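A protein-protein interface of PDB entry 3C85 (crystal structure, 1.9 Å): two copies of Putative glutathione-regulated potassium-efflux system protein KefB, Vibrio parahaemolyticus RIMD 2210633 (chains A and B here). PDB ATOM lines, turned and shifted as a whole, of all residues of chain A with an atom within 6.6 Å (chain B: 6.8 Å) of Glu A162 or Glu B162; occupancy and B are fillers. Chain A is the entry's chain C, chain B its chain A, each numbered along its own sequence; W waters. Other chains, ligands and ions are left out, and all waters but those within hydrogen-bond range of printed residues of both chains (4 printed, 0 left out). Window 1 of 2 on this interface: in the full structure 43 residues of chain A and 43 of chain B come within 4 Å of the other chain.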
ATOM      1  N   ARG A  49      -3.670  20.828  29.002  1.00  0.00           N
ATOM      2  CA  ARG A  49      -4.336  19.855  28.095  1.00  0.00           C
ATOM      3  C   ARG A  49      -5.228  18.857  28.832  1.00  0.00           C
ATOM      4  O   ARG A  49      -6.289  18.463  28.338  1.00  0.00           O
ATOM      5  CB  ARG A  49      -3.335  19.169  27.137  1.00  0.00           C
ATOM      6  CG  ARG A  49      -2.702  20.203  26.209  1.00  0.00           C
ATOM      7  CD  ARG A  49      -1.857  19.607  25.078  1.00  0.00           C
ATOM      8  NE  ARG A  49      -1.566  20.657  24.100  1.00  0.00           N
ATOM      9  CZ  ARG A  49      -0.486  21.428  24.103  1.00  0.00           C
ATOM     10  NH1 ARG A  49       0.482  21.250  25.002  1.00  0.00           N
ATOM     11  NH2 ARG A  49      -0.371  22.377  23.177  1.00  0.00           N
ATOM     12  N   GLY A  53      -9.205  18.624  28.265  1.00  0.00           N
ATOM     13  CA  GLY A  53      -9.796  17.346  27.805  1.00  0.00           C
ATOM     14  C   GLY A  53     -10.997  16.990  28.664  1.00  0.00           C
ATOM     15  O   GLY A  53     -12.063  16.609  28.150  1.00  0.00           O
ATOM     16  N   ILE A 138      -6.261  13.612  39.079  1.00  0.00           N
ATOM     17  CA  ILE A 138      -5.471  12.828  38.149  1.00  0.00           C
ATOM     18  C   ILE A 138      -4.007  13.123  38.462  1.00  0.00           C
ATOM     19  O   ILE A 138      -3.644  14.284  38.689  1.00  0.00           O
ATOM     20  CB  ILE A 138      -5.881  13.092  36.682  1.00  0.00           C
ATOM     21  CG1 ILE A 138      -5.307  12.015  35.737  1.00  0.00           C
ATOM     22  CG2 ILE A 138      -5.564  14.581  36.248  1.00  0.00           C
ATOM     23  CD1 ILE A 138      -5.903  12.067  34.313  1.00  0.00           C
ATOM     24  N   PHE A 157      -6.866   8.869  39.559  1.00  0.00           N
ATOM     25  CA  PHE A 157      -6.512   8.220  38.304  1.00  0.00           C
ATOM     26  C   PHE A 157      -5.111   8.577  37.868  1.00  0.00           C
ATOM     27  O   PHE A 157      -4.591   9.643  38.207  1.00  0.00           O
ATOM     28  CB  PHE A 157      -7.505   8.648  37.227  1.00  0.00           C
ATOM     29  CG  PHE A 157      -8.941   8.347  37.601  1.00  0.00           C
ATOM     30  CD1 PHE A 157      -9.509   7.138  37.302  1.00  0.00           C
ATOM     31  CD2 PHE A 157      -9.701   9.276  38.302  1.00  0.00           C
ATOM     32  CE1 PHE A 157     -10.822   6.867  37.677  1.00  0.00           C
ATOM     33  CE2 PHE A 157     -11.010   8.995  38.676  1.00  0.00           C
ATOM     34  CZ  PHE A 157     -11.565   7.802  38.346  1.00  0.00           C
ATOM     35  N   ASN A 158      -4.530   7.697  37.072  1.00  0.00           N
ATOM     36  CA  ASN A 158      -3.206   7.898  36.522  1.00  0.00           C
ATOM     37  C   ASN A 158      -3.302   8.516  35.126  1.00  0.00           C
ATOM     38  O   ASN A 158      -4.064   8.031  34.268  1.00  0.00           O
ATOM     39  CB  ASN A 158      -2.447   6.564  36.474  1.00  0.00           C
ATOM     40  CG  ASN A 158      -1.079   6.713  35.846  1.00  0.00           C
ATOM     41  OD1 ASN A 158      -0.922   6.568  34.628  1.00  0.00           O
ATOM     42  ND2 ASN A 158      -0.094   7.063  36.654  1.00  0.00           N
ATOM     43  N   ILE A 159      -2.561   9.586  34.893  1.00  0.00           N
ATOM     44  CA  ILE A 159      -2.601  10.276  33.586  1.00  0.00           C
ATOM     45  C   ILE A 159      -2.455   9.335  32.373  1.00  0.00           C
ATOM     46  O   ILE A 159      -3.211   9.399  31.390  1.00  0.00           O
ATOM     47  CB  ILE A 159      -1.465  11.328  33.485  1.00  0.00           C
ATOM     48  CG1 ILE A 159      -1.673  12.468  34.507  1.00  0.00           C
ATOM     49  CG2 ILE A 159      -1.344  11.893  32.017  1.00  0.00           C
ATOM     50  CD1 ILE A 159      -0.540  13.494  34.518  1.00  0.00           C
ATOM     51  N   TYR A 160      -1.450   8.489  32.424  1.00  0.00           N
ATOM     52  CA  TYR A 160      -1.102   7.669  31.268  1.00  0.00           C
ATOM     53  C   TYR A 160      -2.034   6.495  31.027  1.00  0.00           C
ATOM     54  O   TYR A 160      -2.291   6.147  29.881  1.00  0.00           O
ATOM     55  CB  TYR A 160       0.333   7.209  31.395  1.00  0.00           C
ATOM     56  CG  TYR A 160       1.248   8.385  31.558  1.00  0.00           C
ATOM     57  CD1 TYR A 160       1.330   9.366  30.569  1.00  0.00           C
ATOM     58  CD2 TYR A 160       2.012   8.540  32.691  1.00  0.00           C
ATOM     59  CE1 TYR A 160       2.147  10.465  30.707  1.00  0.00           C
ATOM     60  CE2 TYR A 160       2.853   9.651  32.828  1.00  0.00           C
ATOM     61  CZ  TYR A 160       2.903  10.600  31.821  1.00  0.00           C
ATOM     62  OH  TYR A 160       3.701  11.715  31.955  1.00  0.00           O
ATOM     63  N   SER A 161      -2.541   5.877  32.092  1.00  0.00           N
ATOM     64  CA  SER A 161      -3.539   4.819  31.957  1.00  0.00           C
ATOM     65  C   SER A 161      -4.822   5.371  31.361  1.00  0.00           C
ATOM     66  O   SER A 161      -5.398   4.770  30.460  1.00  0.00           O
ATOM     67  CB  SER A 161      -3.832   4.220  33.320  1.00  0.00           C
ATOM     68  OG  SER A 161      -2.630   3.641  33.797  1.00  0.00           O
ATOM     69  N   GLU A 162      -5.242   6.540  31.839  1.00  0.00           N
ATOM     70  CA  GLU A 162      -6.388   7.239  31.233  1.00  0.00           C
ATOM     71  C   GLU A 162      -6.134   7.603  29.759  1.00  0.00           C
ATOM     72  O   GLU A 162      -7.031   7.483  28.920  1.00  0.00           O
ATOM     73  CB  GLU A 162      -6.756   8.484  32.052  1.00  0.00           C
ATOM     74  CG  GLU A 162      -7.252   8.101  33.459  1.00  0.00           C
ATOM     75  CD  GLU A 162      -8.426   7.194  33.384  1.00  0.00           C
ATOM     76  OE1 GLU A 162      -9.391   7.501  32.667  1.00  0.00           O
ATOM     77  OE2 GLU A 162      -8.398   6.151  34.030  1.00  0.00           O
ATOM     78  N   ALA A 163      -4.916   8.050  29.441  1.00  0.00           N
ATOM     79  CA  ALA A 163      -4.581   8.428  28.075  1.00  0.00           C
ATOM     80  C   ALA A 163      -4.680   7.219  27.159  1.00  0.00           C
ATOM     81  O   ALA A 163      -5.143   7.347  26.023  1.00  0.00           O
ATOM     82  CB  ALA A 163      -3.176   8.988  28.020  1.00  0.00           C
ATOM     83  N   GLY A 164      -4.271   6.044  27.637  1.00  0.00           N
ATOM     84  CA  GLY A 164      -4.279   4.849  26.774  1.00  0.00           C
ATOM     85  C   GLY A 164      -5.703   4.389  26.474  1.00  0.00           C
ATOM     86  O   GLY A 164      -6.037   3.979  25.357  1.00  0.00           O
ATOM     87  N   SER A 165      -6.536   4.418  27.492  1.00  0.00           N
ATOM     88  CA  SER A 165      -7.938   4.120  27.313  1.00  0.00           C
ATOM     89  C   SER A 165      -8.632   5.071  26.315  1.00  0.00           C
ATOM     90  O   SER A 165      -9.326   4.611  25.403  1.00  0.00           O
ATOM     91  CB  SER A 165      -8.609   4.184  28.699  1.00  0.00           C
ATOM     92  OG  SER A 165     -10.003   4.297  28.569  1.00  0.00           O
ATOM     93  N   GLY A 166      -8.443   6.383  26.489  1.00  0.00           N
ATOM     94  CA  GLY A 166      -8.990   7.399  25.595  1.00  0.00           C
ATOM     95  C   GLY A 166      -8.455   7.281  24.185  1.00  0.00           C
ATOM     96  O   GLY A 166      -9.198   7.406  23.212  1.00  0.00           O
ATOM     97  N   PHE A 167      -7.158   7.069  24.072  1.00  0.00           N
ATOM     98  CA  PHE A 167      -6.526   6.838  22.811  1.00  0.00           C
ATOM     99  C   PHE A 167      -7.226   5.702  22.036  1.00  0.00           C
ATOM    100  O   PHE A 167      -7.613   5.882  20.882  1.00  0.00           O
ATOM    101  CB  PHE A 167      -5.056   6.534  23.089  1.00  0.00           C
ATOM    102  CG  PHE A 167      -4.223   6.236  21.877  1.00  0.00           C
ATOM    103  CD1 PHE A 167      -4.353   6.963  20.697  1.00  0.00           C
ATOM    104  CD2 PHE A 167      -3.200   5.296  21.970  1.00  0.00           C
ATOM    105  CE1 PHE A 167      -3.511   6.704  19.598  1.00  0.00           C
ATOM    106  CE2 PHE A 167      -2.341   5.034  20.875  1.00  0.00           C
ATOM    107  CZ  PHE A 167      -2.506   5.755  19.684  1.00  0.00           C
ATOM    108  N   ALA A 168      -7.425   4.551  22.672  1.00  0.00           N
ATOM    109  CA  ALA A 168      -8.012   3.432  21.960  1.00  0.00           C
ATOM    110  C   ALA A 168      -9.438   3.756  21.508  1.00  0.00           C
ATOM    111  O   ALA A 168      -9.840   3.408  20.376  1.00  0.00           O
ATOM    112  CB  ALA A 168      -7.955   2.135  22.803  1.00  0.00           C
ATOM    113  N   ARG A 169     -10.204   4.428  22.359  1.00  0.00           N
ATOM    114  CA  ARG A 169     -11.578   4.778  21.984  1.00  0.00           C
ATOM    115  C   ARG A 169     -11.604   5.758  20.826  1.00  0.00           C
ATOM    116  O   ARG A 169     -12.304   5.523  19.834  1.00  0.00           O
ATOM    117  CB  ARG A 169     -12.367   5.344  23.169  1.00  0.00           C
ATOM    118  CG  ARG A 169     -12.744   4.306  24.168  1.00  0.00           C
ATOM    119  CD  ARG A 169     -13.877   4.760  25.092  1.00  0.00           C
ATOM    120  NE  ARG A 169     -14.075   3.772  26.147  1.00  0.00           N
ATOM    121  CZ  ARG A 169     -15.042   2.860  26.188  1.00  0.00           C
ATOM    122  NH1 ARG A 169     -15.951   2.791  25.226  1.00  0.00           N
ATOM    123  NH2 ARG A 169     -15.103   2.019  27.213  1.00  0.00           N
ATOM    124  N   HIS A 170     -10.840   6.844  20.953  1.00  0.00           N
ATOM    125  CA  HIS A 170     -10.812   7.900  19.929  1.00  0.00           C
ATOM    126  C   HIS A 170     -10.304   7.342  18.568  1.00  0.00           C
ATOM    127  O   HIS A 170     -10.789   7.724  17.516  1.00  0.00           O
ATOM    128  CB  HIS A 170      -9.925   9.063  20.392  1.00  0.00           C
ATOM    129  CG  HIS A 170     -10.446  10.434  20.022  1.00  0.00           C
ATOM    130  ND1 HIS A 170      -9.972  11.596  20.604  1.00  0.00           N
ATOM    131  CD2 HIS A 170     -11.412  10.821  19.150  1.00  0.00           C
ATOM    132  CE1 HIS A 170     -10.615  12.635  20.102  1.00  0.00           C
ATOM    133  NE2 HIS A 170     -11.498  12.193  19.217  1.00  0.00           N
ATOM    134  N   VAL A 171      -9.336   6.429  18.596  1.00  0.00           N
ATOM    135  CA  VAL A 171      -8.883   5.774  17.355  1.00  0.00           C
ATOM    136  C   VAL A 171      -9.968   4.949  16.684  1.00  0.00           C
ATOM    137  O   VAL A 171     -10.148   5.014  15.455  1.00  0.00           O
ATOM    138  CB  VAL A 171      -7.646   4.879  17.571  1.00  0.00           C
ATOM    139  CG1 VAL A 171      -7.291   4.173  16.248  1.00  0.00           C
ATOM    140  CG2 VAL A 171      -6.479   5.715  18.006  1.00  0.00           C
ATOM    141  N   ARG B  49       2.405   2.499  30.419  1.00  0.00           N
ATOM    142  CA  ARG B  49       1.067   2.750  30.865  1.00  0.00           C
ATOM    143  C   ARG B  49       0.087   3.126  29.750  1.00  0.00           C
ATOM    144  O   ARG B  49      -1.016   2.716  29.771  1.00  0.00           O
ATOM    145  CB  ARG B  49       1.064   3.750  32.023  1.00  0.00           C
ATOM    146  CG  ARG B  49       1.711   3.218  33.287  1.00  0.00           C
ATOM    147  CD  ARG B  49       1.423   4.053  34.485  1.00  0.00           C
ATOM    148  NE  ARG B  49       0.098   3.786  34.966  1.00  0.00           N
ATOM    149  CZ  ARG B  49      -0.204   2.826  35.814  1.00  0.00           C
ATOM    150  NH1 ARG B  49       0.746   2.055  36.286  1.00  0.00           N
ATOM    151  NH2 ARG B  49      -1.442   2.653  36.194  1.00  0.00           N
ATOM    152  N   GLY B  53      -3.142   0.704  28.797  1.00  0.00           N
ATOM    153  CA  GLY B  53      -4.519   1.154  28.802  1.00  0.00           C
ATOM    154  C   GLY B  53      -5.226   0.933  27.487  1.00  0.00           C
ATOM    155  O   GLY B  53      -6.410   0.591  27.455  1.00  0.00           O
ATOM    156  N   ILE B 138       0.316   8.689  19.444  1.00  0.00           N
ATOM    157  CA  ILE B 138      -0.018   9.551  20.545  1.00  0.00           C
ATOM    158  C   ILE B 138       1.244  10.264  20.915  1.00  0.00           C
ATOM    159  O   ILE B 138       2.273   9.700  20.879  1.00  0.00           O
ATOM    160  CB  ILE B 138      -0.600   8.762  21.726  1.00  0.00           C
ATOM    161  CG1 ILE B 138      -1.372   9.639  22.692  1.00  0.00           C
ATOM    162  CG2 ILE B 138       0.431   7.929  22.392  1.00  0.00           C
ATOM    163  CD1 ILE B 138      -2.239   8.887  23.576  1.00  0.00           C
ATOM    164  N   ALA B 156      -3.745  10.981  14.999  1.00  0.00           N
ATOM    165  CA  ALA B 156      -2.752  11.332  16.006  1.00  0.00           C
ATOM    166  C   ALA B 156      -3.440  12.057  17.161  1.00  0.00           C
ATOM    167  O   ALA B 156      -4.174  13.009  16.914  1.00  0.00           O
ATOM    168  CB  ALA B 156      -1.693  12.234  15.359  1.00  0.00           C
ATOM    169  N   PHE B 157      -3.185  11.633  18.411  1.00  0.00           N
ATOM    170  CA  PHE B 157      -3.923  12.153  19.553  1.00  0.00           C
ATOM    171  C   PHE B 157      -2.958  12.621  20.587  1.00  0.00           C
ATOM    172  O   PHE B 157      -1.812  12.182  20.635  1.00  0.00           O
ATOM    173  CB  PHE B 157      -4.844  11.063  20.102  1.00  0.00           C
ATOM    174  CG  PHE B 157      -5.950  10.717  19.145  1.00  0.00           C
ATOM    175  CD1 PHE B 157      -6.978  11.655  18.882  1.00  0.00           C
ATOM    176  CD2 PHE B 157      -5.945   9.501  18.476  1.00  0.00           C
ATOM    177  CE1 PHE B 157      -7.981  11.368  17.990  1.00  0.00           C
ATOM    178  CE2 PHE B 157      -6.968   9.194  17.567  1.00  0.00           C
ATOM    179  CZ  PHE B 157      -7.984  10.134  17.337  1.00  0.00           C
ATOM    180  N   ASN B 158      -3.386  13.546  21.403  1.00  0.00           N
ATOM    181  CA  ASN B 158      -2.472  14.110  22.395  1.00  0.00           C
ATOM    182  C   ASN B 158      -2.597  13.351  23.714  1.00  0.00           C
ATOM    183  O   ASN B 158      -3.727  13.152  24.194  1.00  0.00           O
ATOM    184  CB  ASN B 158      -2.849  15.588  22.622  1.00  0.00           C
ATOM    185  CG  ASN B 158      -1.904  16.268  23.560  1.00  0.00           C
ATOM    186  OD1 ASN B 158      -1.963  16.045  24.782  1.00  0.00           O
ATOM    187  ND2 ASN B 158      -1.018  17.117  23.009  1.00  0.00           N
ATOM    188  N   ILE B 159      -1.466  12.920  24.293  1.00  0.00           N
ATOM    189  CA  ILE B 159      -1.481  12.108  25.537  1.00  0.00           C
ATOM    190  C   ILE B 159      -2.334  12.782  26.636  1.00  0.00           C
ATOM    191  O   ILE B 159      -3.171  12.136  27.294  1.00  0.00           O
ATOM    192  CB  ILE B 159      -0.052  11.942  26.082  1.00  0.00           C
ATOM    193  CG1 ILE B 159       0.815  11.080  25.155  1.00  0.00           C
ATOM    194  CG2 ILE B 159      -0.040  11.371  27.545  1.00  0.00           C
ATOM    195  CD1 ILE B 159       2.282  11.135  25.537  1.00  0.00           C
ATOM    196  N   TYR B 160      -2.123  14.080  26.845  1.00  0.00           N
ATOM    197  CA  TYR B 160      -2.771  14.796  27.967  1.00  0.00           C
ATOM    198  C   TYR B 160      -4.235  15.139  27.703  1.00  0.00           C
ATOM    199  O   TYR B 160      -5.023  15.081  28.612  1.00  0.00           O
ATOM    200  CB  TYR B 160      -1.952  16.036  28.357  1.00  0.00           C
ATOM    201  CG  TYR B 160      -0.555  15.578  28.666  1.00  0.00           C
ATOM    202  CD1 TYR B 160      -0.269  14.923  29.878  1.00  0.00           C
ATOM    203  CD2 TYR B 160       0.457  15.741  27.733  1.00  0.00           C
ATOM    204  CE1 TYR B 160       0.995  14.442  30.139  1.00  0.00           C
ATOM    205  CE2 TYR B 160       1.743  15.275  27.990  1.00  0.00           C
ATOM    206  CZ  TYR B 160       1.989  14.624  29.183  1.00  0.00           C
ATOM    207  OH  TYR B 160       3.243  14.168  29.393  1.00  0.00           O
ATOM    208  N   SER B 161      -4.591  15.455  26.455  1.00  0.00           N
ATOM    209  CA  SER B 161      -6.002  15.630  26.085  1.00  0.00           C
ATOM    210  C   SER B 161      -6.793  14.364  26.308  1.00  0.00           C
ATOM    211  O   SER B 161      -7.891  14.387  26.875  1.00  0.00           O
ATOM    212  CB  SER B 161      -6.116  16.047  24.608  1.00  0.00           C
ATOM    213  OG  SER B 161      -5.431  17.281  24.405  1.00  0.00           O
ATOM    214  N   GLU B 162      -6.245  13.255  25.831  1.00  0.00           N
ATOM    215  CA  GLU B 162      -6.856  11.928  26.011  1.00  0.00           C
ATOM    216  C   GLU B 162      -6.978  11.573  27.491  1.00  0.00           C
ATOM    217  O   GLU B 162      -8.021  11.054  27.927  1.00  0.00           O
ATOM    218  CB  GLU B 162      -6.031  10.855  25.257  1.00  0.00           C
ATOM    219  CG  GLU B 162      -6.076  11.045  23.700  1.00  0.00           C
ATOM    220  CD  GLU B 162      -7.512  11.112  23.156  1.00  0.00           C
ATOM    221  OE1 GLU B 162      -8.365  10.282  23.563  1.00  0.00           O
ATOM    222  OE2 GLU B 162      -7.796  12.001  22.314  1.00  0.00           O
ATOM    223  N   ALA B 163      -5.925  11.826  28.255  1.00  0.00           N
ATOM    224  CA  ALA B 163      -5.991  11.639  29.708  1.00  0.00           C
ATOM    225  C   ALA B 163      -7.177  12.394  30.360  1.00  0.00           C
ATOM    226  O   ALA B 163      -7.909  11.812  31.135  1.00  0.00           O
ATOM    227  CB  ALA B 163      -4.681  12.045  30.356  1.00  0.00           C
ATOM    228  N   GLY B 164      -7.351  13.669  30.039  1.00  0.00           N
ATOM    229  CA  GLY B 164      -8.425  14.488  30.606  1.00  0.00           C
ATOM    230  C   GLY B 164      -9.792  13.981  30.200  1.00  0.00           C
ATOM    231  O   GLY B 164     -10.740  13.930  31.038  1.00  0.00           O
ATOM    232  N   SER B 165      -9.909  13.594  28.929  1.00  0.00           N
ATOM    233  CA  SER B 165     -11.158  12.987  28.424  1.00  0.00           C
ATOM    234  C   SER B 165     -11.558  11.710  29.192  1.00  0.00           C
ATOM    235  O   SER B 165     -12.705  11.584  29.691  1.00  0.00           O
ATOM    236  CB  SER B 165     -10.997  12.665  26.913  1.00  0.00           C
ATOM    237  OG  SER B 165     -12.075  11.834  26.512  1.00  0.00           O
ATOM    238  N   GLY B 166     -10.610  10.774  29.321  1.00  0.00           N
ATOM    239  CA  GLY B 166     -10.859   9.507  29.998  1.00  0.00           C
ATOM    240  C   GLY B 166     -11.059   9.751  31.485  1.00  0.00           C
ATOM    241  O   GLY B 166     -11.894   9.113  32.088  1.00  0.00           O
ATOM    242  N   PHE B 167     -10.286  10.677  32.071  1.00  0.00           N
ATOM    243  CA  PHE B 167     -10.459  11.136  33.477  1.00  0.00           C
ATOM    244  C   PHE B 167     -11.923  11.504  33.764  1.00  0.00           C
ATOM    245  O   PHE B 167     -12.561  10.930  34.678  1.00  0.00           O
ATOM    246  CB  PHE B 167      -9.482  12.296  33.732  1.00  0.00           C
ATOM    247  CG  PHE B 167      -9.574  12.968  35.111  1.00  0.00           C
ATOM    248  CD1 PHE B 167      -9.755  12.227  36.299  1.00  0.00           C
ATOM    249  CD2 PHE B 167      -9.396  14.330  35.208  1.00  0.00           C
ATOM    250  CE1 PHE B 167      -9.836  12.852  37.533  1.00  0.00           C
ATOM    251  CE2 PHE B 167      -9.468  14.972  36.444  1.00  0.00           C
ATOM    252  CZ  PHE B 167      -9.660  14.241  37.609  1.00  0.00           C
ATOM    253  N   ALA B 168     -12.468  12.426  32.976  1.00  0.00           N
ATOM    254  CA  ALA B 168     -13.820  12.889  33.167  1.00  0.00           C
ATOM    255  C   ALA B 168     -14.823  11.746  32.968  1.00  0.00           C
ATOM    256  O   ALA B 168     -15.704  11.520  33.800  1.00  0.00           O
ATOM    257  CB  ALA B 168     -14.100  14.092  32.211  1.00  0.00           C
ATOM    258  N   ARG B 169     -14.661  11.006  31.883  1.00  0.00           N
ATOM    259  CA  ARG B 169     -15.472   9.813  31.621  1.00  0.00           C
ATOM    260  C   ARG B 169     -15.514   8.798  32.802  1.00  0.00           C
ATOM    261  O   ARG B 169     -16.610   8.376  33.266  1.00  0.00           O
ATOM    262  CB  ARG B 169     -15.013   9.193  30.288  1.00  0.00           C
ATOM    263  CG  ARG B 169     -15.905   8.135  29.776  1.00  0.00           C
ATOM    264  CD  ARG B 169     -15.535   7.716  28.367  1.00  0.00           C
ATOM    265  NE  ARG B 169     -16.347   6.542  28.089  1.00  0.00           N
ATOM    266  CZ  ARG B 169     -15.970   5.319  28.421  1.00  0.00           C
ATOM    267  NH1 ARG B 169     -14.764   5.130  28.973  1.00  0.00           N
ATOM    268  NH2 ARG B 169     -16.773   4.289  28.171  1.00  0.00           N
ATOM    269  N   HIS B 170     -14.370   8.410  33.310  1.00  0.00           N
ATOM    270  CA  HIS B 170     -14.322   7.498  34.402  1.00  0.00           C
ATOM    271  C   HIS B 170     -14.804   8.028  35.739  1.00  0.00           C
ATOM    272  O   HIS B 170     -15.368   7.308  36.497  1.00  0.00           O
ATOM    273  CB  HIS B 170     -12.979   6.832  34.498  1.00  0.00           C
ATOM    274  CG  HIS B 170     -12.638   6.006  33.296  1.00  0.00           C
ATOM    275  ND1 HIS B 170     -11.428   6.087  32.656  1.00  0.00           N
ATOM    276  CD2 HIS B 170     -13.358   5.090  32.616  1.00  0.00           C
ATOM    277  CE1 HIS B 170     -11.413   5.249  31.643  1.00  0.00           C
ATOM    278  NE2 HIS B 170     -12.569   4.629  31.601  1.00  0.00           N
ATOM    279  N   VAL B 171     -14.577   9.302  35.985  1.00  0.00           N
ATOM    280  CA  VAL B 171     -15.093   9.942  37.201  1.00  0.00           C
ATOM    281  C   VAL B 171     -16.615   9.866  37.153  1.00  0.00           C
ATOM    282  O   VAL B 171     -17.238   9.491  38.133  1.00  0.00           O
ATOM    283  CB  VAL B 171     -14.628  11.421  37.340  1.00  0.00           C
ATOM    284  CG1 VAL B 171     -15.309  12.156  38.490  1.00  0.00           C
ATOM    285  CG2 VAL B 171     -13.140  11.482  37.549  1.00  0.00           C
HETATM  286  O   HOH W   1     -11.120  10.105  23.223  1.00  0.00           O
HETATM  287  O   HOH W   2      -2.077   1.455  32.125  1.00  0.00           O
HETATM  288  O   HOH W   3      -6.866  19.136  25.665  1.00  0.00           O
HETATM  289  O   HOH W   4     -11.912   6.647  28.193  1.00  0.00           O
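The backbone carbonyl oxygen (O) of Gly A166 lies close to the side-chain carboxylate (OE1) of Glu B162.
The side-chain carboxylate (OE2) of Glu B162 lies within hydrogen-bond range of a ring nitrogen (ND1) of His A170 (2.8 Å).
NH2 of Arg A169 sits close to NH2 of Arg B169 (3.0 Å).
The guanidinium group (NE) of Arg B49 lies within hydrogen-bond range of the side-chain amide oxygen (OD1) of Asn A158.
The guanidinium group (NH2) of Arg B49 lies within hydrogen-bond range of the side-chain hydroxyl (OG) of Ser A161.
The side-chain carboxylate (OE1) of Glu B162 sits at hydrogen-bond distance from the backbone NH (N) of Phe A167 (3.5 Å).
O of Gly B166 lies close to OE1 of Glu A162.
The backbone NH of Phe B167 sits at hydrogen-bond distance from the side-chain carboxylate of Glu A162, at 3.4 Å.
A ring nitrogen (ND1) of His B170 sits at hydrogen-bond distance from the side-chain carboxylate (OE1) of Glu A162 (2.5 Å).
A ring nitrogen (NE2) of His B170 is in hydrogen-bond range of the guanidinium group of Arg B169 (3.5 Å).
The backbone NH (N) of Tyr A160 sits at hydrogen-bond distance from the side-chain amide oxygen (OD1) of Asn A158 (3.0 Å).
OD1 of Asn B158 sits at hydrogen-bond distance from N of Tyr B160, 2.9 Å away.
O of Gly B166 lies within hydrogen-bond range of ND1 of His B170.
The backbone NH (N) of Ser B161 is in hydrogen-bond range of the side-chain amide oxygen (OD1) of Asn B158 (3.2 Å).
The side-chain amide oxygen (OD1) of Asn A158 sits at hydrogen-bond distance from the backbone NH (N) of Ser A161 (3.1 Å).
Asn B158 touches Arg A49.
Gly A53 touches Gly B164.
N of Ser B165 touches C of Gly A53, 3.6 Å away.
Phe A157 touches Phe B167 (CD2 to CD1, 3.6 Å).
Tyr B160 touches Ile A159.
Ala B163 touches Ala A163 (N to CA, 3.7 Å).
N of Ser A165 touches C of Gly B53, at 3.7 Å.
His B170 touches Ser A165 (CE1 to OG, 3.5 Å).
Phe A167 touches Ile B138 (CB to CD1, 3.7 Å).
Phe A167 touches Phe B157 (CD1 to CD2, 3.7 Å).
Of the printed residues of chain A, Arg B49 touches Asn A158, Tyr A160 and Ser A161.
Ala B156 touches none of the printed residues of chain A.
Of the printed residues of chain A, Ile B159 touches Tyr A160 and Ala A163.
Of chain A, only Glu A162 (3.8 Å), Ala A163 (3.7 Å), Gly A166 (3.0 Å), Phe A167 (3.5 Å) and His A170 (2.8 Å) come within 4 Å of Glu B162.
The nearest printed residue of chain B that does not touch Ile A159 is Ile B159 (4.7 Å).
Hydrophobic or aromatic side chains of chain B that line the printed part of chain A: Ile B138, Phe B157, Ile B159, Tyr B160, Ala B163, Phe B167, His B170 and Val B171.
Along chain B the printed residues that touch a printed residue of chain A span positions 49 to 171.
Among the printed residues, no Asp or Glu carboxylate lies within 4 Å of a Lys or Arg side-chain nitrogen of the other chain.
Gly A53 touches Gly B164, and with the chains exchanged Gly A164 touches Gly B53.
Phe A157 touches His B170, and with the chains exchanged His A170 touches Phe B157.
Ile A159 touches Tyr B160, and with the chains exchanged Tyr A160 touches Ile B159.
Arg B169 touches its own counterpart, Arg A169.
18 positions are printed for both chains.
Of the 37 pairs that touch across the chains among the printed residues, 34 have their exchanged pair printed and touching as well.
Water W3 bridges OG of Ser B161 and O of Arg A49.
Water W1 lies within hydrogen-bond range of the side-chain carboxylate of Glu B162 (2.8 Å), a ring nitrogen (ND1) of His A170 (3.2 Å) and the backbone carbonyl oxygen of Gly A166 (3.3 Å).
Water W2 lies within hydrogen-bond range of OG of Ser A161 and O of Arg B49.
Water W4 lies within hydrogen-bond range of OG of Ser A165 (3.1 Å) and NH1 of Arg B169 (3.3 Å).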
